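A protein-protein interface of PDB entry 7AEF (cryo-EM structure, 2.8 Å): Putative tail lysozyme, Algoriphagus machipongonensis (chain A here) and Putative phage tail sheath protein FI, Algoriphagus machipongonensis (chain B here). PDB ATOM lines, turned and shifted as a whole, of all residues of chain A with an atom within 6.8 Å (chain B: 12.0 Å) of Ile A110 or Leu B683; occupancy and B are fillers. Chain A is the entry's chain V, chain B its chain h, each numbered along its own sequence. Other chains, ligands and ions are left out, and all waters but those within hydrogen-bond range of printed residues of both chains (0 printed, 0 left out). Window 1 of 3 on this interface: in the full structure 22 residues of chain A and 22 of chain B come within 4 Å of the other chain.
Ile A80 touches none of the printed residues of chain B. No residue of chain B comes within 4 Å of Ile A96. No residue of chain B comes within 4 Å of Asp A97. No residue of chain B comes within 4 Å of Ile A98. No residue of chain B comes within 4 Å of Thr A99. Of chain B, only Phe B680, Ile B681 and Ile B682 come within 4 Å of Leu A108. Of chain B, only Ile B682 (3.0 Å), Leu B683 (3.5 Å) and Lys B684 (3.2 Å) come within 4 Å of Ile A110. His A111 touches just these residues of chain B: Lys B684 (3.8 Å) and Ser B686 (3.4 Å). Leu A112 touches just these residues of chain B: Lys B684, Phe B685 and Ser B686. Of the printed residues of chain A, Phe B680 touches Leu A108 (2.9 Å). Printed residues of chain A within 4 Å of Ile B682: Leu A108, Leu A109 and Ile A110. Of the printed residues of chain A, Ser B686 touches His A111 (3.4 Å) and Leu A112 (3.1 Å). The nearest residue of chain B that does not touch Ile A110 is Ile B681 (4.04 Å). The nearest residue of chain A that does not touch Leu B683 is Phe A43 (4.1 Å). The nearest printed residue of chain A that does not touch Ile B681 is Ile A110 (4.04 Å).
The backbone carbonyl oxygen (O) of Phe B680 lies within hydrogen-bond range of the backbone NH (N) of Leu A108, at 2.9 Å. The backbone carbonyl oxygen (O) of Leu A108 lies within hydrogen-bond range of the backbone NH (N) of Ile B682, 3.0 Å away. N of Ile A110 lies within hydrogen-bond range of O of Ile B682 (3.0 Å). The backbone carbonyl oxygen of Ile A110 lies within hydrogen-bond range of the backbone NH of Lys B684, 3.2 Å away. OG of Ser B686 is in hydrogen-bond range of NE2 of His A111, 3.4 Å away. The backbone NH (N) of Leu A112 is in hydrogen-bond range of the backbone carbonyl oxygen (O) of Lys B684 (3.0 Å). O of Leu A112 sits at hydrogen-bond distance from N of Ser B686 (3.1 Å).
The backbone carbonyl oxygen of Asp A97 sits at hydrogen-bond distance from the backbone NH of His A111, at 2.9 Å. The backbone carbonyl oxygen of Thr A99 sits at hydrogen-bond distance from the backbone NH of Leu A109, 2.8 Å away.
Among the printed residues, merely in contact across the chains: Leu A112 with Phe B685 (3.4 Å), Ile A110 with Leu B683 (3.5 Å), Leu A108 with Ile B681 (3.6 Å), Leu A109 with Ile B682 (3.8 Å) and His A111 with Lys B684 (3.8 Å).
Hydrophobic or aromatic side chains of chain A within 4 Å of the printed part of chain B: Leu A108, Leu A109, Ile A110, His A111 and Leu A112. Hydrophobic or aromatic side chains of chain B that line the printed part of chain A: Ile B682, Leu B683 and Phe B685.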
ATOM      1  N   LEU A  39      23.806 -28.536  31.369  1.00  0.00           N
ATOM      2  CA  LEU A  39      24.436 -27.267  31.033  1.00  0.00           C
ATOM      3  C   LEU A  39      23.415 -26.146  30.912  1.00  0.00           C
ATOM      4  O   LEU A  39      23.661 -25.036  31.396  1.00  0.00           O
ATOM      5  CB  LEU A  39      25.232 -27.408  29.738  1.00  0.00           C
ATOM      6  CG  LEU A  39      26.519 -28.234  29.801  1.00  0.00           C
ATOM      7  CD1 LEU A  39      27.031 -28.496  28.402  1.00  0.00           C
ATOM      8  CD2 LEU A  39      27.582 -27.515  30.632  1.00  0.00           C
ATOM      9  N   PHE A  43      23.645 -22.686  33.586  1.00  0.00           N
ATOM     10  CA  PHE A  43      23.845 -21.317  33.150  1.00  0.00           C
ATOM     11  C   PHE A  43      22.557 -20.512  33.097  1.00  0.00           C
ATOM     12  O   PHE A  43      22.571 -19.373  32.638  1.00  0.00           O
ATOM     13  CB  PHE A  43      24.576 -21.313  31.812  1.00  0.00           C
ATOM     14  CG  PHE A  43      26.026 -21.690  31.947  1.00  0.00           C
ATOM     15  CD1 PHE A  43      26.475 -22.971  31.650  1.00  0.00           C
ATOM     16  CD2 PHE A  43      26.934 -20.765  32.422  1.00  0.00           C
ATOM     17  CE1 PHE A  43      27.807 -23.300  31.811  1.00  0.00           C
ATOM     18  CE2 PHE A  43      28.258 -21.089  32.582  1.00  0.00           C
ATOM     19  CZ  PHE A  43      28.695 -22.353  32.282  1.00  0.00           C
ATOM     20  N   SER A  44      21.458 -21.080  33.559  1.00  0.00           N
ATOM     21  CA  SER A  44      20.203 -20.377  33.732  1.00  0.00           C
ATOM     22  C   SER A  44      19.890 -19.981  35.148  1.00  0.00           C
ATOM     23  O   SER A  44      18.832 -19.388  35.377  1.00  0.00           O
ATOM     24  CB  SER A  44      19.016 -21.146  33.136  1.00  0.00           C
ATOM     25  OG  SER A  44      19.254 -21.565  31.819  1.00  0.00           O
ATOM     26  N   LEU A  60      27.262 -14.601  34.935  1.00  0.00           N
ATOM     27  CA  LEU A  60      27.405 -13.944  33.633  1.00  0.00           C
ATOM     28  C   LEU A  60      26.680 -12.591  33.543  1.00  0.00           C
ATOM     29  O   LEU A  60      27.153 -11.702  32.833  1.00  0.00           O
ATOM     30  CB  LEU A  60      26.931 -14.875  32.523  1.00  0.00           C
ATOM     31  CG  LEU A  60      27.821 -16.089  32.212  1.00  0.00           C
ATOM     32  CD1 LEU A  60      27.104 -16.998  31.244  1.00  0.00           C
ATOM     33  CD2 LEU A  60      29.178 -15.677  31.626  1.00  0.00           C
ATOM     34  N   VAL A  76      35.115 -13.491  30.946  1.00  0.00           N
ATOM     35  CA  VAL A  76      34.016 -14.395  30.570  1.00  0.00           C
ATOM     36  C   VAL A  76      34.483 -15.834  30.556  1.00  0.00           C
ATOM     37  O   VAL A  76      33.802 -16.733  31.063  1.00  0.00           O
ATOM     38  CB  VAL A  76      33.457 -14.056  29.178  1.00  0.00           C
ATOM     39  CG1 VAL A  76      32.480 -15.128  28.712  1.00  0.00           C
ATOM     40  CG2 VAL A  76      32.762 -12.822  29.173  1.00  0.00           C
ATOM     41  N   ILE A  80      33.092 -19.126  32.947  1.00  0.00           N
ATOM     42  CA  ILE A  80      32.523 -20.339  32.377  1.00  0.00           C
ATOM     43  C   ILE A  80      33.307 -21.558  32.820  1.00  0.00           C
ATOM     44  O   ILE A  80      32.718 -22.560  33.238  1.00  0.00           O
ATOM     45  CB  ILE A  80      32.469 -20.246  30.844  1.00  0.00           C
ATOM     46  CG1 ILE A  80      31.446 -19.188  30.447  1.00  0.00           C
ATOM     47  CG2 ILE A  80      32.142 -21.618  30.212  1.00  0.00           C
ATOM     48  CD1 ILE A  80      31.483 -18.788  29.003  1.00  0.00           C
ATOM     49  N   ILE A  96      36.205 -21.987  23.785  1.00  0.00           N
ATOM     50  CA  ILE A  96      35.220 -20.939  24.007  1.00  0.00           C
ATOM     51  C   ILE A  96      35.479 -19.815  23.014  1.00  0.00           C
ATOM     52  O   ILE A  96      36.546 -19.192  23.033  1.00  0.00           O
ATOM     53  CB  ILE A  96      35.234 -20.436  25.458  1.00  0.00           C
ATOM     54  CG1 ILE A  96      34.931 -21.607  26.400  1.00  0.00           C
ATOM     55  CG2 ILE A  96      34.204 -19.323  25.636  1.00  0.00           C
ATOM     56  CD1 ILE A  96      35.133 -21.342  27.877  1.00  0.00           C
ATOM     57  N   ASP A  97      34.507 -19.558  22.151  1.00  0.00           N
ATOM     58  CA  ASP A  97      34.610 -18.578  21.075  1.00  0.00           C
ATOM     59  C   ASP A  97      33.651 -17.398  21.358  1.00  0.00           C
ATOM     60  O   ASP A  97      32.426 -17.553  21.281  1.00  0.00           O
ATOM     61  CB  ASP A  97      34.252 -19.264  19.757  1.00  0.00           C
ATOM     62  CG  ASP A  97      34.595 -18.442  18.559  1.00  0.00           C
ATOM     63  OD1 ASP A  97      34.619 -17.215  18.655  1.00  0.00           O
ATOM     64  OD2 ASP A  97      34.573 -18.977  17.447  1.00  0.00           O
ATOM     65  N   ILE A  98      34.196 -16.206  21.623  1.00  0.00           N
ATOM     66  CA  ILE A  98      33.393 -15.031  21.994  1.00  0.00           C
ATOM     67  C   ILE A  98      33.459 -13.960  20.908  1.00  0.00           C
ATOM     68  O   ILE A  98      34.531 -13.395  20.661  1.00  0.00           O
ATOM     69  CB  ILE A  98      33.844 -14.435  23.329  1.00  0.00           C
ATOM     70  CG1 ILE A  98      33.765 -15.491  24.417  1.00  0.00           C
ATOM     71  CG2 ILE A  98      32.975 -13.232  23.666  1.00  0.00           C
ATOM     72  CD1 ILE A  98      34.415 -15.104  25.691  1.00  0.00           C
ATOM     73  N   THR A  99      32.313 -13.654  20.281  1.00  0.00           N
ATOM     74  CA  THR A  99      32.255 -12.675  19.183  1.00  0.00           C
ATOM     75  C   THR A  99      31.017 -11.761  19.208  1.00  0.00           C
ATOM     76  O   THR A  99      30.007 -12.056  19.843  1.00  0.00           O
ATOM     77  CB  THR A  99      32.328 -13.365  17.810  1.00  0.00           C
ATOM     78  OG1 THR A  99      32.279 -12.377  16.775  1.00  0.00           O
ATOM     79  CG2 THR A  99      31.183 -14.345  17.631  1.00  0.00           C
ATOM     80  N   LEU A 108      26.086 -10.082  22.347  1.00  0.00           N
ATOM     81  CA  LEU A 108      27.354 -10.768  22.519  1.00  0.00           C
ATOM     82  C   LEU A 108      27.075 -12.240  22.277  1.00  0.00           C
ATOM     83  O   LEU A 108      26.125 -12.787  22.837  1.00  0.00           O
ATOM     84  CB  LEU A 108      27.927 -10.531  23.925  1.00  0.00           C
ATOM     85  CG  LEU A 108      29.282 -11.155  24.291  1.00  0.00           C
ATOM     86  CD1 LEU A 108      30.381 -10.530  23.473  1.00  0.00           C
ATOM     87  CD2 LEU A 108      29.586 -10.972  25.769  1.00  0.00           C
ATOM     88  N   LEU A 109      27.870 -12.881  21.431  1.00  0.00           N
ATOM     89  CA  LEU A 109      27.624 -14.270  21.051  1.00  0.00           C
ATOM     90  C   LEU A 109      28.711 -15.182  21.604  1.00  0.00           C
ATOM     91  O   LEU A 109      29.887 -15.024  21.266  1.00  0.00           O
ATOM     92  CB  LEU A 109      27.578 -14.388  19.537  1.00  0.00           C
ATOM     93  CG  LEU A 109      26.591 -13.472  18.827  1.00  0.00           C
ATOM     94  CD1 LEU A 109      26.772 -13.627  17.332  1.00  0.00           C
ATOM     95  CD2 LEU A 109      25.162 -13.777  19.233  1.00  0.00           C
ATOM     96  N   ILE A 110      28.331 -16.159  22.418  1.00  0.00           N
ATOM     97  CA  ILE A 110      29.315 -17.054  23.018  1.00  0.00           C
ATOM     98  C   ILE A 110      29.048 -18.490  22.591  1.00  0.00           C
ATOM     99  O   ILE A 110      27.975 -19.034  22.869  1.00  0.00           O
ATOM    100  CB  ILE A 110      29.325 -16.947  24.547  1.00  0.00           C
ATOM    101  CG1 ILE A 110      29.608 -15.501  24.955  1.00  0.00           C
ATOM    102  CG2 ILE A 110      30.378 -17.899  25.114  1.00  0.00           C
ATOM    103  CD1 ILE A 110      29.437 -15.202  26.408  1.00  0.00           C
ATOM    104  N   HIS A 111      30.040 -19.127  21.982  1.00  0.00           N
ATOM    105  CA  HIS A 111      29.916 -20.515  21.535  1.00  0.00           C
ATOM    106  C   HIS A 111      30.851 -21.433  22.329  1.00  0.00           C
ATOM    107  O   HIS A 111      32.077 -21.330  22.219  1.00  0.00           O
ATOM    108  CB  HIS A 111      30.181 -20.590  20.034  1.00  0.00           C
ATOM    109  CG  HIS A 111      30.004 -21.949  19.428  1.00  0.00           C
ATOM    110  ND1 HIS A 111      30.465 -22.236  18.163  1.00  0.00           N
ATOM    111  CD2 HIS A 111      29.418 -23.081  19.881  1.00  0.00           C
ATOM    112  CE1 HIS A 111      30.176 -23.490  17.866  1.00  0.00           C
ATOM    113  NE2 HIS A 111      29.543 -24.026  18.892  1.00  0.00           N
ATOM    114  N   LEU A 112      30.272 -22.344  23.114  1.00  0.00           N
ATOM    115  CA  LEU A 112      31.027 -23.307  23.916  1.00  0.00           C
ATOM    116  C   LEU A 112      31.049 -24.675  23.254  1.00  0.00           C
ATOM    117  O   LEU A 112      29.996 -25.268  23.009  1.00  0.00           O
ATOM    118  CB  LEU A 112      30.450 -23.478  25.325  1.00  0.00           C
ATOM    119  CG  LEU A 112      31.037 -24.625  26.204  1.00  0.00           C
ATOM    120  CD1 LEU A 112      32.492 -24.384  26.567  1.00  0.00           C
ATOM    121  CD2 LEU A 112      30.221 -24.834  27.476  1.00  0.00           C
ATOM    122  N   ALA B 678      26.519  -3.648  25.171  1.00  0.00           N
ATOM    123  CA  ALA B 678      25.878  -4.935  24.946  1.00  0.00           C
ATOM    124  C   ALA B 678      24.671  -5.088  25.860  1.00  0.00           C
ATOM    125  O   ALA B 678      24.778  -4.856  27.062  1.00  0.00           O
ATOM    126  CB  ALA B 678      26.850  -6.070  25.202  1.00  0.00           C
ATOM    127  N   GLU B 679      23.542  -5.525  25.307  1.00  0.00           N
ATOM    128  CA  GLU B 679      22.344  -5.760  26.109  1.00  0.00           C
ATOM    129  C   GLU B 679      21.960  -7.226  26.221  1.00  0.00           C
ATOM    130  O   GLU B 679      21.270  -7.601  27.169  1.00  0.00           O
ATOM    131  CB  GLU B 679      21.145  -4.979  25.549  1.00  0.00           C
ATOM    132  CG  GLU B 679      21.235  -3.468  25.668  1.00  0.00           C
ATOM    133  CD  GLU B 679      20.026  -2.743  25.073  1.00  0.00           C
ATOM    134  OE1 GLU B 679      19.867  -2.782  23.867  1.00  0.00           O
ATOM    135  OE2 GLU B 679      19.268  -2.118  25.800  1.00  0.00           O
ATOM    136  N   PHE B 680      22.371  -8.055  25.279  1.00  0.00           N
ATOM    137  CA  PHE B 680      21.928  -9.435  25.268  1.00  0.00           C
ATOM    138  C   PHE B 680      23.105 -10.378  25.159  1.00  0.00           C
ATOM    139  O   PHE B 680      24.087 -10.073  24.492  1.00  0.00           O
ATOM    140  CB  PHE B 680      20.995  -9.668  24.091  1.00  0.00           C
ATOM    141  CG  PHE B 680      19.839  -8.739  24.077  1.00  0.00           C
ATOM    142  CD1 PHE B 680      19.849  -7.642  23.252  1.00  0.00           C
ATOM    143  CD2 PHE B 680      18.770  -8.919  24.912  1.00  0.00           C
ATOM    144  CE1 PHE B 680      18.813  -6.757  23.247  1.00  0.00           C
ATOM    145  CE2 PHE B 680      17.731  -8.026  24.908  1.00  0.00           C
ATOM    146  CZ  PHE B 680      17.757  -6.947  24.075  1.00  0.00           C
ATOM    147  N   ILE B 681      22.981 -11.542  25.786  1.00  0.00           N
ATOM    148  CA  ILE B 681      23.987 -12.589  25.705  1.00  0.00           C
ATOM    149  C   ILE B 681      23.357 -13.865  25.206  1.00  0.00           C
ATOM    150  O   ILE B 681      22.405 -14.367  25.802  1.00  0.00           O
ATOM    151  CB  ILE B 681      24.652 -12.840  27.063  1.00  0.00           C
ATOM    152  CG1 ILE B 681      25.350 -11.554  27.524  1.00  0.00           C
ATOM    153  CG2 ILE B 681      25.615 -14.040  26.978  1.00  0.00           C
ATOM    154  CD1 ILE B 681      25.862 -11.577  28.930  1.00  0.00           C
ATOM    155  N   ILE B 682      23.902 -14.416  24.139  1.00  0.00           N
ATOM    156  CA  ILE B 682      23.366 -15.632  23.564  1.00  0.00           C
ATOM    157  C   ILE B 682      24.383 -16.755  23.649  1.00  0.00           C
ATOM    158  O   ILE B 682      25.503 -16.619  23.160  1.00  0.00           O
ATOM    159  CB  ILE B 682      22.944 -15.384  22.117  1.00  0.00           C
ATOM    160  CG1 ILE B 682      21.875 -14.279  22.107  1.00  0.00           C
ATOM    161  CG2 ILE B 682      22.432 -16.678  21.495  1.00  0.00           C
ATOM    162  CD1 ILE B 682      21.535 -13.741  20.761  1.00  0.00           C
ATOM    163  N   LEU B 683      23.991 -17.867  24.256  1.00  0.00           N
ATOM    164  CA  LEU B 683      24.868 -19.017  24.391  1.00  0.00           C
ATOM    165  C   LEU B 683      24.469 -20.150  23.471  1.00  0.00           C
ATOM    166  O   LEU B 683      23.295 -20.321  23.154  1.00  0.00           O
ATOM    167  CB  LEU B 683      24.851 -19.556  25.808  1.00  0.00           C
ATOM    168  CG  LEU B 683      25.227 -18.599  26.915  1.00  0.00           C
ATOM    169  CD1 LEU B 683      25.073 -19.316  28.220  1.00  0.00           C
ATOM    170  CD2 LEU B 683      26.644 -18.110  26.741  1.00  0.00           C
ATOM    171  N   LYS B 684      25.466 -20.939  23.083  1.00  0.00           N
ATOM    172  CA  LYS B 684      25.275 -22.130  22.270  1.00  0.00           C
ATOM    173  C   LYS B 684      26.239 -23.211  22.750  1.00  0.00           C
ATOM    174  O   LYS B 684      27.374 -22.911  23.119  1.00  0.00           O
ATOM    175  CB  LYS B 684      25.515 -21.815  20.792  1.00  0.00           C
ATOM    176  CG  LYS B 684      25.343 -23.010  19.867  1.00  0.00           C
ATOM    177  CD  LYS B 684      25.601 -22.634  18.423  1.00  0.00           C
ATOM    178  CE  LYS B 684      25.444 -23.835  17.502  1.00  0.00           C
ATOM    179  NZ  LYS B 684      24.073 -24.411  17.573  1.00  0.00           N
ATOM    180  N   PHE B 685      25.799 -24.465  22.748  1.00  0.00           N
ATOM    181  CA  PHE B 685      26.645 -25.578  23.151  1.00  0.00           C
ATOM    182  C   PHE B 685      26.710 -26.646  22.073  1.00  0.00           C
ATOM    183  O   PHE B 685      25.720 -26.888  21.414  1.00  0.00           O
ATOM    184  CB  PHE B 685      26.103 -26.270  24.396  1.00  0.00           C
ATOM    185  CG  PHE B 685      25.876 -25.374  25.561  1.00  0.00           C
ATOM    186  CD1 PHE B 685      24.601 -25.174  26.052  1.00  0.00           C
ATOM    187  CD2 PHE B 685      26.928 -24.766  26.197  1.00  0.00           C
ATOM    188  CE1 PHE B 685      24.381 -24.357  27.133  1.00  0.00           C
ATOM    189  CE2 PHE B 685      26.711 -23.945  27.280  1.00  0.00           C
ATOM    190  CZ  PHE B 685      25.437 -23.738  27.744  1.00  0.00           C
ATOM    191  N   SER B 686      27.867 -27.293  21.901  1.00  0.00           N
ATOM    192  CA  SER B 686      27.989 -28.415  20.986  1.00  0.00           C
ATOM    193  C   SER B 686      29.031 -29.368  21.564  1.00  0.00           C
ATOM    194  O   SER B 686      29.909 -28.960  22.322  1.00  0.00           O
ATOM    195  CB  SER B 686      28.440 -27.979  19.604  1.00  0.00           C
ATOM    196  OG  SER B 686      29.696 -27.375  19.641  1.00  0.00           O
ATOM    197  N   HIS B 687      28.966 -30.623  21.153  1.00  0.00           N
ATOM    198  CA  HIS B 687      29.827 -31.647  21.701  1.00  0.00           C
ATOM    199  C   HIS B 687      30.423 -32.592  20.675  1.00  0.00           C
ATOM    200  O   HIS B 687      29.959 -32.697  19.556  1.00  0.00           O
ATOM    201  CB  HIS B 687      29.010 -32.495  22.641  1.00  0.00           C
ATOM    202  CG  HIS B 687      28.316 -33.624  21.957  1.00  0.00           C
ATOM    203  ND1 HIS B 687      27.104 -33.476  21.322  1.00  0.00           N
ATOM    204  CD2 HIS B 687      28.662 -34.926  21.809  1.00  0.00           C
ATOM    205  CE1 HIS B 687      26.742 -34.630  20.796  1.00  0.00           C
ATOM    206  NE2 HIS B 687      27.670 -35.526  21.079  1.00  0.00           N
